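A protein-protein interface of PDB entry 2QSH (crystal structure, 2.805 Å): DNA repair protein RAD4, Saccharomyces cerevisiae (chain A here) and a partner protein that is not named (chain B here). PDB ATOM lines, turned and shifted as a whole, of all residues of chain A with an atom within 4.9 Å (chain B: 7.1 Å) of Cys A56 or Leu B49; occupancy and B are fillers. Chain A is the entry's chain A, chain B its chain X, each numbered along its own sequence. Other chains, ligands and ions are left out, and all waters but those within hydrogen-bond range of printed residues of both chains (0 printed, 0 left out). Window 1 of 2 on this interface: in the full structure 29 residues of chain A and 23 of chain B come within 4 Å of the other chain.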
ATOM      1  N   LEU A  52      35.885 -11.788  23.514  1.00  0.00           N
ATOM      2  CA  LEU A  52      35.268 -11.379  22.251  1.00  0.00           C
ATOM      3  C   LEU A  52      33.897 -10.755  22.496  1.00  0.00           C
ATOM      4  O   LEU A  52      33.580  -9.678  21.993  1.00  0.00           O
ATOM      5  CB  LEU A  52      35.116 -12.590  21.323  1.00  0.00           C
ATOM      6  CG  LEU A  52      35.359 -12.463  19.810  1.00  0.00           C
ATOM      7  CD1 LEU A  52      34.834 -13.693  19.108  1.00  0.00           C
ATOM      8  CD2 LEU A  52      34.733 -11.224  19.187  1.00  0.00           C
ATOM      9  N   TYR A  53      33.103 -11.446  23.301  1.00  0.00           N
ATOM     10  CA  TYR A  53      31.763 -11.029  23.629  1.00  0.00           C
ATOM     11  C   TYR A  53      31.795  -9.715  24.394  1.00  0.00           C
ATOM     12  O   TYR A  53      31.070  -8.783  24.037  1.00  0.00           O
ATOM     13  CB  TYR A  53      31.104 -12.115  24.451  1.00  0.00           C
ATOM     14  CG  TYR A  53      29.601 -12.198  24.364  1.00  0.00           C
ATOM     15  CD1 TYR A  53      28.981 -13.300  23.781  1.00  0.00           C
ATOM     16  CD2 TYR A  53      28.797 -11.205  24.918  1.00  0.00           C
ATOM     17  CE1 TYR A  53      27.594 -13.393  23.733  1.00  0.00           C
ATOM     18  CE2 TYR A  53      27.418 -11.283  24.878  1.00  0.00           C
ATOM     19  CZ  TYR A  53      26.817 -12.374  24.286  1.00  0.00           C
ATOM     20  OH  TYR A  53      25.439 -12.437  24.259  1.00  0.00           O
ATOM     21  N   LEU A  54      32.643  -9.633  25.424  1.00  0.00           N
ATOM     22  CA  LEU A  54      32.818  -8.389  26.193  1.00  0.00           C
ATOM     23  C   LEU A  54      33.108  -7.189  25.278  1.00  0.00           C
ATOM     24  O   LEU A  54      32.431  -6.156  25.351  1.00  0.00           O
ATOM     25  CB  LEU A  54      33.953  -8.524  27.209  1.00  0.00           C
ATOM     26  CG  LEU A  54      33.841  -7.867  28.601  1.00  0.00           C
ATOM     27  CD1 LEU A  54      35.232  -7.561  29.184  1.00  0.00           C
ATOM     28  CD2 LEU A  54      32.945  -6.624  28.666  1.00  0.00           C
ATOM     29  N   VAL A  55      34.105  -7.339  24.411  1.00  0.00           N
ATOM     30  CA  VAL A  55      34.507  -6.267  23.510  1.00  0.00           C
ATOM     31  C   VAL A  55      33.313  -5.774  22.690  1.00  0.00           C
ATOM     32  O   VAL A  55      33.072  -4.564  22.585  1.00  0.00           O
ATOM     33  CB  VAL A  55      35.645  -6.728  22.572  1.00  0.00           C
ATOM     34  CG1 VAL A  55      36.079  -5.605  21.650  1.00  0.00           C
ATOM     35  CG2 VAL A  55      36.817  -7.216  23.388  1.00  0.00           C
ATOM     36  N   CYS A  56      32.558  -6.713  22.127  1.00  0.00           N
ATOM     37  CA  CYS A  56      31.396  -6.368  21.326  1.00  0.00           C
ATOM     38  C   CYS A  56      30.363  -5.586  22.129  1.00  0.00           C
ATOM     39  O   CYS A  56      29.848  -4.583  21.647  1.00  0.00           O
ATOM     40  CB  CYS A  56      30.800  -7.623  20.692  1.00  0.00           C
ATOM     41  SG  CYS A  56      31.905  -8.350  19.432  1.00  0.00           S
ATOM     42  N   LEU A  57      30.091  -6.029  23.357  1.00  0.00           N
ATOM     43  CA  LEU A  57      29.153  -5.345  24.252  1.00  0.00           C
ATOM     44  C   LEU A  57      29.634  -3.937  24.582  1.00  0.00           C
ATOM     45  O   LEU A  57      28.857  -2.984  24.537  1.00  0.00           O
ATOM     46  CB  LEU A  57      28.920  -6.144  25.545  1.00  0.00           C
ATOM     47  CG  LEU A  57      28.082  -7.434  25.483  1.00  0.00           C
ATOM     48  CD1 LEU A  57      28.276  -8.268  26.740  1.00  0.00           C
ATOM     49  CD2 LEU A  57      26.592  -7.160  25.242  1.00  0.00           C
ATOM     50  N   MET A  58      30.919  -3.808  24.899  1.00  0.00           N
ATOM     51  CA  MET A  58      31.487  -2.507  25.219  1.00  0.00           C
ATOM     52  C   MET A  58      31.448  -1.587  24.012  1.00  0.00           C
ATOM     53  O   MET A  58      31.157  -0.397  24.147  1.00  0.00           O
ATOM     54  CB  MET A  58      32.899  -2.648  25.775  1.00  0.00           C
ATOM     55  CG  MET A  58      32.909  -3.289  27.160  1.00  0.00           C
ATOM     56  SD  MET A  58      34.550  -3.541  27.855  1.00  0.00           S
ATOM     57  CE  MET A  58      34.961  -1.873  28.363  1.00  0.00           C
ATOM     58  N   VAL A  59      31.703  -2.140  22.830  1.00  0.00           N
ATOM     59  CA  VAL A  59      31.587  -1.356  21.608  1.00  0.00           C
ATOM     60  C   VAL A  59      30.137  -0.962  21.356  1.00  0.00           C
ATOM     61  O   VAL A  59      29.865   0.154  20.901  1.00  0.00           O
ATOM     62  CB  VAL A  59      32.190  -2.079  20.403  1.00  0.00           C
ATOM     63  CG1 VAL A  59      31.868  -1.351  19.103  1.00  0.00           C
ATOM     64  CG2 VAL A  59      33.693  -2.184  20.583  1.00  0.00           C
ATOM     65  N   HIS A  60      29.203  -1.858  21.673  1.00  0.00           N
ATOM     66  CA  HIS A  60      27.792  -1.515  21.543  1.00  0.00           C
ATOM     67  C   HIS A  60      27.401  -0.331  22.433  1.00  0.00           C
ATOM     68  O   HIS A  60      26.651   0.543  22.006  1.00  0.00           O
ATOM     69  CB  HIS A  60      26.876  -2.693  21.839  1.00  0.00           C
ATOM     70  CG  HIS A  60      25.429  -2.312  21.854  1.00  0.00           C
ATOM     71  ND1 HIS A  60      24.671  -2.299  23.004  1.00  0.00           N
ATOM     72  CD2 HIS A  60      24.616  -1.871  20.865  1.00  0.00           C
ATOM     73  CE1 HIS A  60      23.443  -1.906  22.717  1.00  0.00           C
ATOM     74  NE2 HIS A  60      23.385  -1.636  21.424  1.00  0.00           N
ATOM     75  N   LEU B  38      28.581  -7.779  11.284  1.00  0.00           N
ATOM     76  CA  LEU B  38      29.171  -7.564  12.598  1.00  0.00           C
ATOM     77  C   LEU B  38      28.879  -6.161  13.096  1.00  0.00           C
ATOM     78  O   LEU B  38      28.472  -5.981  14.232  1.00  0.00           O
ATOM     79  CB  LEU B  38      30.680  -7.783  12.548  1.00  0.00           C
ATOM     80  CG  LEU B  38      31.354  -8.631  13.627  1.00  0.00           C
ATOM     81  CD1 LEU B  38      32.792  -8.192  13.792  1.00  0.00           C
ATOM     82  CD2 LEU B  38      30.639  -8.550  14.957  1.00  0.00           C
ATOM     83  N   VAL B  41      25.000  -5.863  13.857  1.00  0.00           N
ATOM     84  CA  VAL B  41      24.661  -6.556  15.090  1.00  0.00           C
ATOM     85  C   VAL B  41      25.180  -5.774  16.300  1.00  0.00           C
ATOM     86  O   VAL B  41      24.423  -5.470  17.215  1.00  0.00           O
ATOM     87  CB  VAL B  41      25.210  -7.994  15.089  1.00  0.00           C
ATOM     88  CG1 VAL B  41      25.193  -8.593  16.495  1.00  0.00           C
ATOM     89  CG2 VAL B  41      24.408  -8.859  14.132  1.00  0.00           C
ATOM     90  N   VAL B  42      26.462  -5.427  16.289  1.00  0.00           N
ATOM     91  CA  VAL B  42      27.054  -4.663  17.386  1.00  0.00           C
ATOM     92  C   VAL B  42      26.294  -3.361  17.636  1.00  0.00           C
ATOM     93  O   VAL B  42      26.027  -3.021  18.776  1.00  0.00           O
ATOM     94  CB  VAL B  42      28.570  -4.378  17.159  1.00  0.00           C
ATOM     95  CG1 VAL B  42      29.067  -3.318  18.099  1.00  0.00           C
ATOM     96  CG2 VAL B  42      29.390  -5.633  17.364  1.00  0.00           C
ATOM     97  N   SER B  43      25.931  -2.642  16.580  1.00  0.00           N
ATOM     98  CA  SER B  43      25.337  -1.326  16.757  1.00  0.00           C
ATOM     99  C   SER B  43      23.859  -1.338  17.148  1.00  0.00           C
ATOM    100  O   SER B  43      23.452  -0.610  18.051  1.00  0.00           O
ATOM    101  CB  SER B  43      25.552  -0.456  15.519  1.00  0.00           C
ATOM    102  OG  SER B  43      24.736  -0.891  14.448  1.00  0.00           O
ATOM    103  N   ASN B  45      21.621  -4.463  17.028  1.00  0.00           N
ATOM    104  CA  ASN B  45      21.026  -5.763  17.296  1.00  0.00           C
ATOM    105  C   ASN B  45      21.920  -6.630  18.199  1.00  0.00           C
ATOM    106  O   ASN B  45      22.208  -7.778  17.853  1.00  0.00           O
ATOM    107  CB  ASN B  45      20.738  -6.493  15.977  1.00  0.00           C
ATOM    108  CG  ASN B  45      19.747  -5.746  15.086  1.00  0.00           C
ATOM    109  OD1 ASN B  45      18.535  -5.912  15.208  1.00  0.00           O
ATOM    110  ND2 ASN B  45      20.264  -4.941  14.162  1.00  0.00           N
ATOM    111  N   PRO B  46      22.348  -6.102  19.372  1.00  0.00           N
ATOM    112  CA  PRO B  46      23.340  -6.874  20.139  1.00  0.00           C
ATOM    113  C   PRO B  46      22.748  -8.132  20.745  1.00  0.00           C
ATOM    114  O   PRO B  46      23.482  -8.992  21.207  1.00  0.00           O
ATOM    115  CB  PRO B  46      23.790  -5.903  21.228  1.00  0.00           C
ATOM    116  CG  PRO B  46      22.636  -4.972  21.409  1.00  0.00           C
ATOM    117  CD  PRO B  46      21.962  -4.854  20.065  1.00  0.00           C
ATOM    118  N   GLU B  47      21.428  -8.238  20.724  1.00  0.00           N
ATOM    119  CA  GLU B  47      20.747  -9.465  21.118  1.00  0.00           C
ATOM    120  C   GLU B  47      21.106 -10.639  20.189  1.00  0.00           C
ATOM    121  O   GLU B  47      20.959 -11.797  20.567  1.00  0.00           O
ATOM    122  CB  GLU B  47      19.224  -9.253  21.169  1.00  0.00           C
ATOM    123  CG  GLU B  47      18.559  -8.869  19.832  1.00  0.00           C
ATOM    124  CD  GLU B  47      18.645  -7.377  19.500  1.00  0.00           C
ATOM    125  OE1 GLU B  47      19.188  -6.589  20.325  1.00  0.00           O
ATOM    126  OE2 GLU B  47      18.162  -6.991  18.407  1.00  0.00           O
ATOM    127  N   ALA B  48      21.589 -10.329  18.986  1.00  0.00           N
ATOM    128  CA  ALA B  48      21.941 -11.348  17.992  1.00  0.00           C
ATOM    129  C   ALA B  48      23.430 -11.698  17.983  1.00  0.00           C
ATOM    130  O   ALA B  48      23.906 -12.383  17.071  1.00  0.00           O
ATOM    131  CB  ALA B  48      21.501 -10.902  16.611  1.00  0.00           C
ATOM    132  N   LEU B  49      24.159 -11.238  18.998  1.00  0.00           N
ATOM    133  CA  LEU B  49      25.592 -11.499  19.084  1.00  0.00           C
ATOM    134  C   LEU B  49      25.934 -12.983  19.136  1.00  0.00           C
ATOM    135  O   LEU B  49      26.696 -13.478  18.303  1.00  0.00           O
ATOM    136  CB  LEU B  49      26.199 -10.794  20.291  1.00  0.00           C
ATOM    137  CG  LEU B  49      26.637  -9.359  20.034  1.00  0.00           C
ATOM    138  CD1 LEU B  49      26.734  -8.620  21.355  1.00  0.00           C
ATOM    139  CD2 LEU B  49      27.959  -9.326  19.280  1.00  0.00           C
ATOM    140  N   ALA B  50      25.359 -13.685  20.107  1.00  0.00           N
ATOM    141  CA  ALA B  50      25.704 -15.079  20.357  1.00  0.00           C
ATOM    142  C   ALA B  50      25.859 -15.951  19.095  1.00  0.00           C
ATOM    143  O   ALA B  50      26.919 -16.554  18.910  1.00  0.00           O
ATOM    144  CB  ALA B  50      24.739 -15.704  21.357  1.00  0.00           C
ATOM    145  N   PRO B  51      24.825 -16.014  18.219  1.00  0.00           N
ATOM    146  CA  PRO B  51      24.989 -16.888  17.047  1.00  0.00           C
ATOM    147  C   PRO B  51      25.985 -16.340  16.026  1.00  0.00           C
ATOM    148  O   PRO B  51      26.711 -17.118  15.401  1.00  0.00           O
ATOM    149  CB  PRO B  51      23.578 -16.959  16.452  1.00  0.00           C
ATOM    150  CG  PRO B  51      22.922 -15.709  16.879  1.00  0.00           C
ATOM    151  CD  PRO B  51      23.503 -15.353  18.225  1.00  0.00           C
ATOM    152  N   LEU B  52      26.019 -15.016  15.875  1.00  0.00           N
ATOM    153  CA  LEU B  52      26.942 -14.360  14.955  1.00  0.00           C
ATOM    154  C   LEU B  52      28.379 -14.630  15.365  1.00  0.00           C
ATOM    155  O   LEU B  52      29.189 -15.045  14.541  1.00  0.00           O
ATOM    156  CB  LEU B  52      26.675 -12.853  14.898  1.00  0.00           C
ATOM    157  CG  LEU B  52      27.095 -12.050  13.656  1.00  0.00           C
ATOM    158  CD1 LEU B  52      28.494 -11.474  13.787  1.00  0.00           C
ATOM    159  CD2 LEU B  52      26.953 -12.860  12.362  1.00  0.00           C
ATOM    160  N   LEU B  53      28.677 -14.414  16.644  1.00  0.00           N
ATOM    161  CA  LEU B  53      30.000 -14.673  17.196  1.00  0.00           C
ATOM    162  C   LEU B  53      30.372 -16.153  17.191  1.00  0.00           C
ATOM    163  O   LEU B  53      31.535 -16.494  16.980  1.00  0.00           O
ATOM    164  CB  LEU B  53      30.111 -14.111  18.609  1.00  0.00           C
ATOM    165  CG  LEU B  53      30.176 -12.594  18.748  1.00  0.00           C
ATOM    166  CD1 LEU B  53      30.240 -12.239  20.218  1.00  0.00           C
ATOM    167  CD2 LEU B  53      31.375 -12.024  18.009  1.00  0.00           C
ATOM    168  N   GLU B  54      29.392 -17.021  17.436  1.00  0.00           N
ATOM    169  CA  GLU B  54      29.576 -18.466  17.286  1.00  0.00           C
ATOM    170  C   GLU B  54      30.001 -18.798  15.865  1.00  0.00           C
ATOM    171  O   GLU B  54      30.994 -19.492  15.651  1.00  0.00           O
ATOM    172  CB  GLU B  54      28.281 -19.220  17.606  1.00  0.00           C
ATOM    173  CG  GLU B  54      28.178 -19.749  19.023  1.00  0.00           C
ATOM    174  CD  GLU B  54      29.021 -20.988  19.242  1.00  0.00           C
ATOM    175  OE1 GLU B  54      30.237 -20.845  19.488  1.00  0.00           O
ATOM    176  OE2 GLU B  54      28.465 -22.105  19.172  1.00  0.00           O
ATOM    177  N   ASN B  55      29.240 -18.281  14.904  1.00  0.00           N
ATOM    178  CA  ASN B  55      29.487 -18.507  13.486  1.00  0.00           C
ATOM    179  C   ASN B  55      30.827 -17.955  12.992  1.00  0.00           C
ATOM    180  O   ASN B  55      31.615 -18.680  12.383  1.00  0.00           O
ATOM    181  CB  ASN B  55      28.327 -17.932  12.660  1.00  0.00           C
ATOM    182  CG  ASN B  55      28.672 -17.769  11.190  1.00  0.00           C
ATOM    183  OD1 ASN B  55      29.138 -18.702  10.538  1.00  0.00           O
ATOM    184  ND2 ASN B  55      28.436 -16.575  10.660  1.00  0.00           N
ATOM    185  N   ILE B  56      31.071 -16.675  13.261  1.00  0.00           N
ATOM    186  CA  ILE B  56      32.234 -15.964  12.731  1.00  0.00           C
ATOM    187  C   ILE B  56      33.575 -16.558  13.184  1.00  0.00           C
ATOM    188  O   ILE B  56      34.480 -16.745  12.370  1.00  0.00           O
ATOM    189  CB  ILE B  56      32.153 -14.445  13.058  1.00  0.00           C
ATOM    190  CG1 ILE B  56      33.093 -13.633  12.174  1.00  0.00           C
ATOM    191  CG2 ILE B  56      32.436 -14.178  14.534  1.00  0.00           C
ATOM    192  CD1 ILE B  56      32.842 -12.155  12.263  1.00  0.00           C
ATOM    193  N   ILE B  67      42.361 -10.936  18.654  1.00  0.00           N
ATOM    194  CA  ILE B  67      41.667 -10.307  19.778  1.00  0.00           C
ATOM    195  C   ILE B  67      42.540 -10.291  21.027  1.00  0.00           C
ATOM    196  O   ILE B  67      42.631  -9.275  21.723  1.00  0.00           O
ATOM    197  CB  ILE B  67      40.340 -11.047  20.095  1.00  0.00           C
ATOM    198  CG1 ILE B  67      39.355 -10.928  18.929  1.00  0.00           C
ATOM    199  CG2 ILE B  67      39.707 -10.533  21.385  1.00  0.00           C
ATOM    200  CD1 ILE B  67      38.682  -9.581  18.798  1.00  0.00           C
ATOM    201  N   PHE B  74      40.896  -4.380  16.637  1.00  0.00           N
ATOM    202  CA  PHE B  74      39.555  -4.892  16.404  1.00  0.00           C
ATOM    203  C   PHE B  74      38.507  -3.826  16.680  1.00  0.00           C
ATOM    204  O   PHE B  74      37.572  -3.660  15.894  1.00  0.00           O
ATOM    205  CB  PHE B  74      39.290  -6.132  17.253  1.00  0.00           C
ATOM    206  CG  PHE B  74      37.994  -6.819  16.930  1.00  0.00           C
ATOM    207  CD1 PHE B  74      36.880  -6.665  17.761  1.00  0.00           C
ATOM    208  CD2 PHE B  74      37.883  -7.622  15.793  1.00  0.00           C
ATOM    209  CE1 PHE B  74      35.679  -7.304  17.470  1.00  0.00           C
ATOM    210  CE2 PHE B  74      36.682  -8.265  15.487  1.00  0.00           C
ATOM    211  CZ  PHE B  74      35.576  -8.105  16.324  1.00  0.00           C
ATOM    212  N   LEU B  78      35.608  -2.024  13.990  1.00  0.00           N
ATOM    213  CA  LEU B  78      34.177  -1.918  14.190  1.00  0.00           C
ATOM    214  C   LEU B  78      33.678  -0.476  14.171  1.00  0.00           C
ATOM    215  O   LEU B  78      32.571  -0.197  13.702  1.00  0.00           O
ATOM    216  CB  LEU B  78      33.797  -2.573  15.504  1.00  0.00           C
ATOM    217  CG  LEU B  78      33.850  -4.090  15.568  1.00  0.00           C
ATOM    218  CD1 LEU B  78      33.612  -4.501  16.994  1.00  0.00           C
ATOM    219  CD2 LEU B  78      32.797  -4.698  14.662  1.00  0.00           C
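The side-chain sulfur (SG) of Cys A56 lies within hydrogen-bond range of the backbone carbonyl oxygen (O) of Leu A52 (3.3 Å).
Of the 9 printed residues of chain A, 5 touch a printed residue of chain B.
Printed residues of chain B that touch a printed residue of chain A: Val B42, Ser B43, Pro B46, Leu B49 and Leu B53.
Hydrophobic or aromatic side chains of chain B within 4 Å of the printed part of chain A: Val B42, Pro B46, Leu B49 and Leu B53.
Along chain B the printed residues that touch a printed residue of chain A span positions 42 to 53.
Among the printed residues, 9 pairs touch across the chains.
Among the printed residues, no Asp or Glu carboxylate lies within 4 Å of a Lys or Arg side-chain nitrogen of the other chain.
Leu A52 touches Leu B53.
CD1 of Leu B53 touches CD1 of Tyr A53, at 3.9 Å.
Cys A56 touches Val B42 (O to CG1, 3.8 Å).
Cys A56 touches Leu B49.
Leu B53 touches Cys A56 (CD2 to SG, 3.98 Å).
Val A59 touches Val B42 (CG1 to CG1, 3.6 Å).
Val B42 touches His A60.
His A60 touches Ser B43.
His A60 touches Pro B46 (NE2 to CG, 3.4 Å).
Printed residues of chain B within 4 Å of Tyr A53: Leu B53.
Of chain B, only Val B42 (3.8 Å), Leu B49 (3.6 Å) and Leu B53 (3.98 Å) come within 4 Å of Cys A56.
Of the printed residues of chain A, Val B42 touches Cys A56, Val A59 and His A60.
Ala B48 touches none of the printed residues of chain A.
Of chain A, only Cys A56 comes within 4 Å of Leu B49.
Printed residues of chain A within 4 Å of Leu B53: Leu A52, Tyr A53 and Cys A56.
Glu B54 touches none of the printed residues of chain A.
The nearest residue of chain B that does not touch Cys A56 is Phe B74 (4.4 Å).
The nearest residue of chain A that does not touch Leu B49 is Leu A57 (4.2 Å).
The nearest printed residue of chain A that does not touch Ser B43 is Val A59 (6.3 Å).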
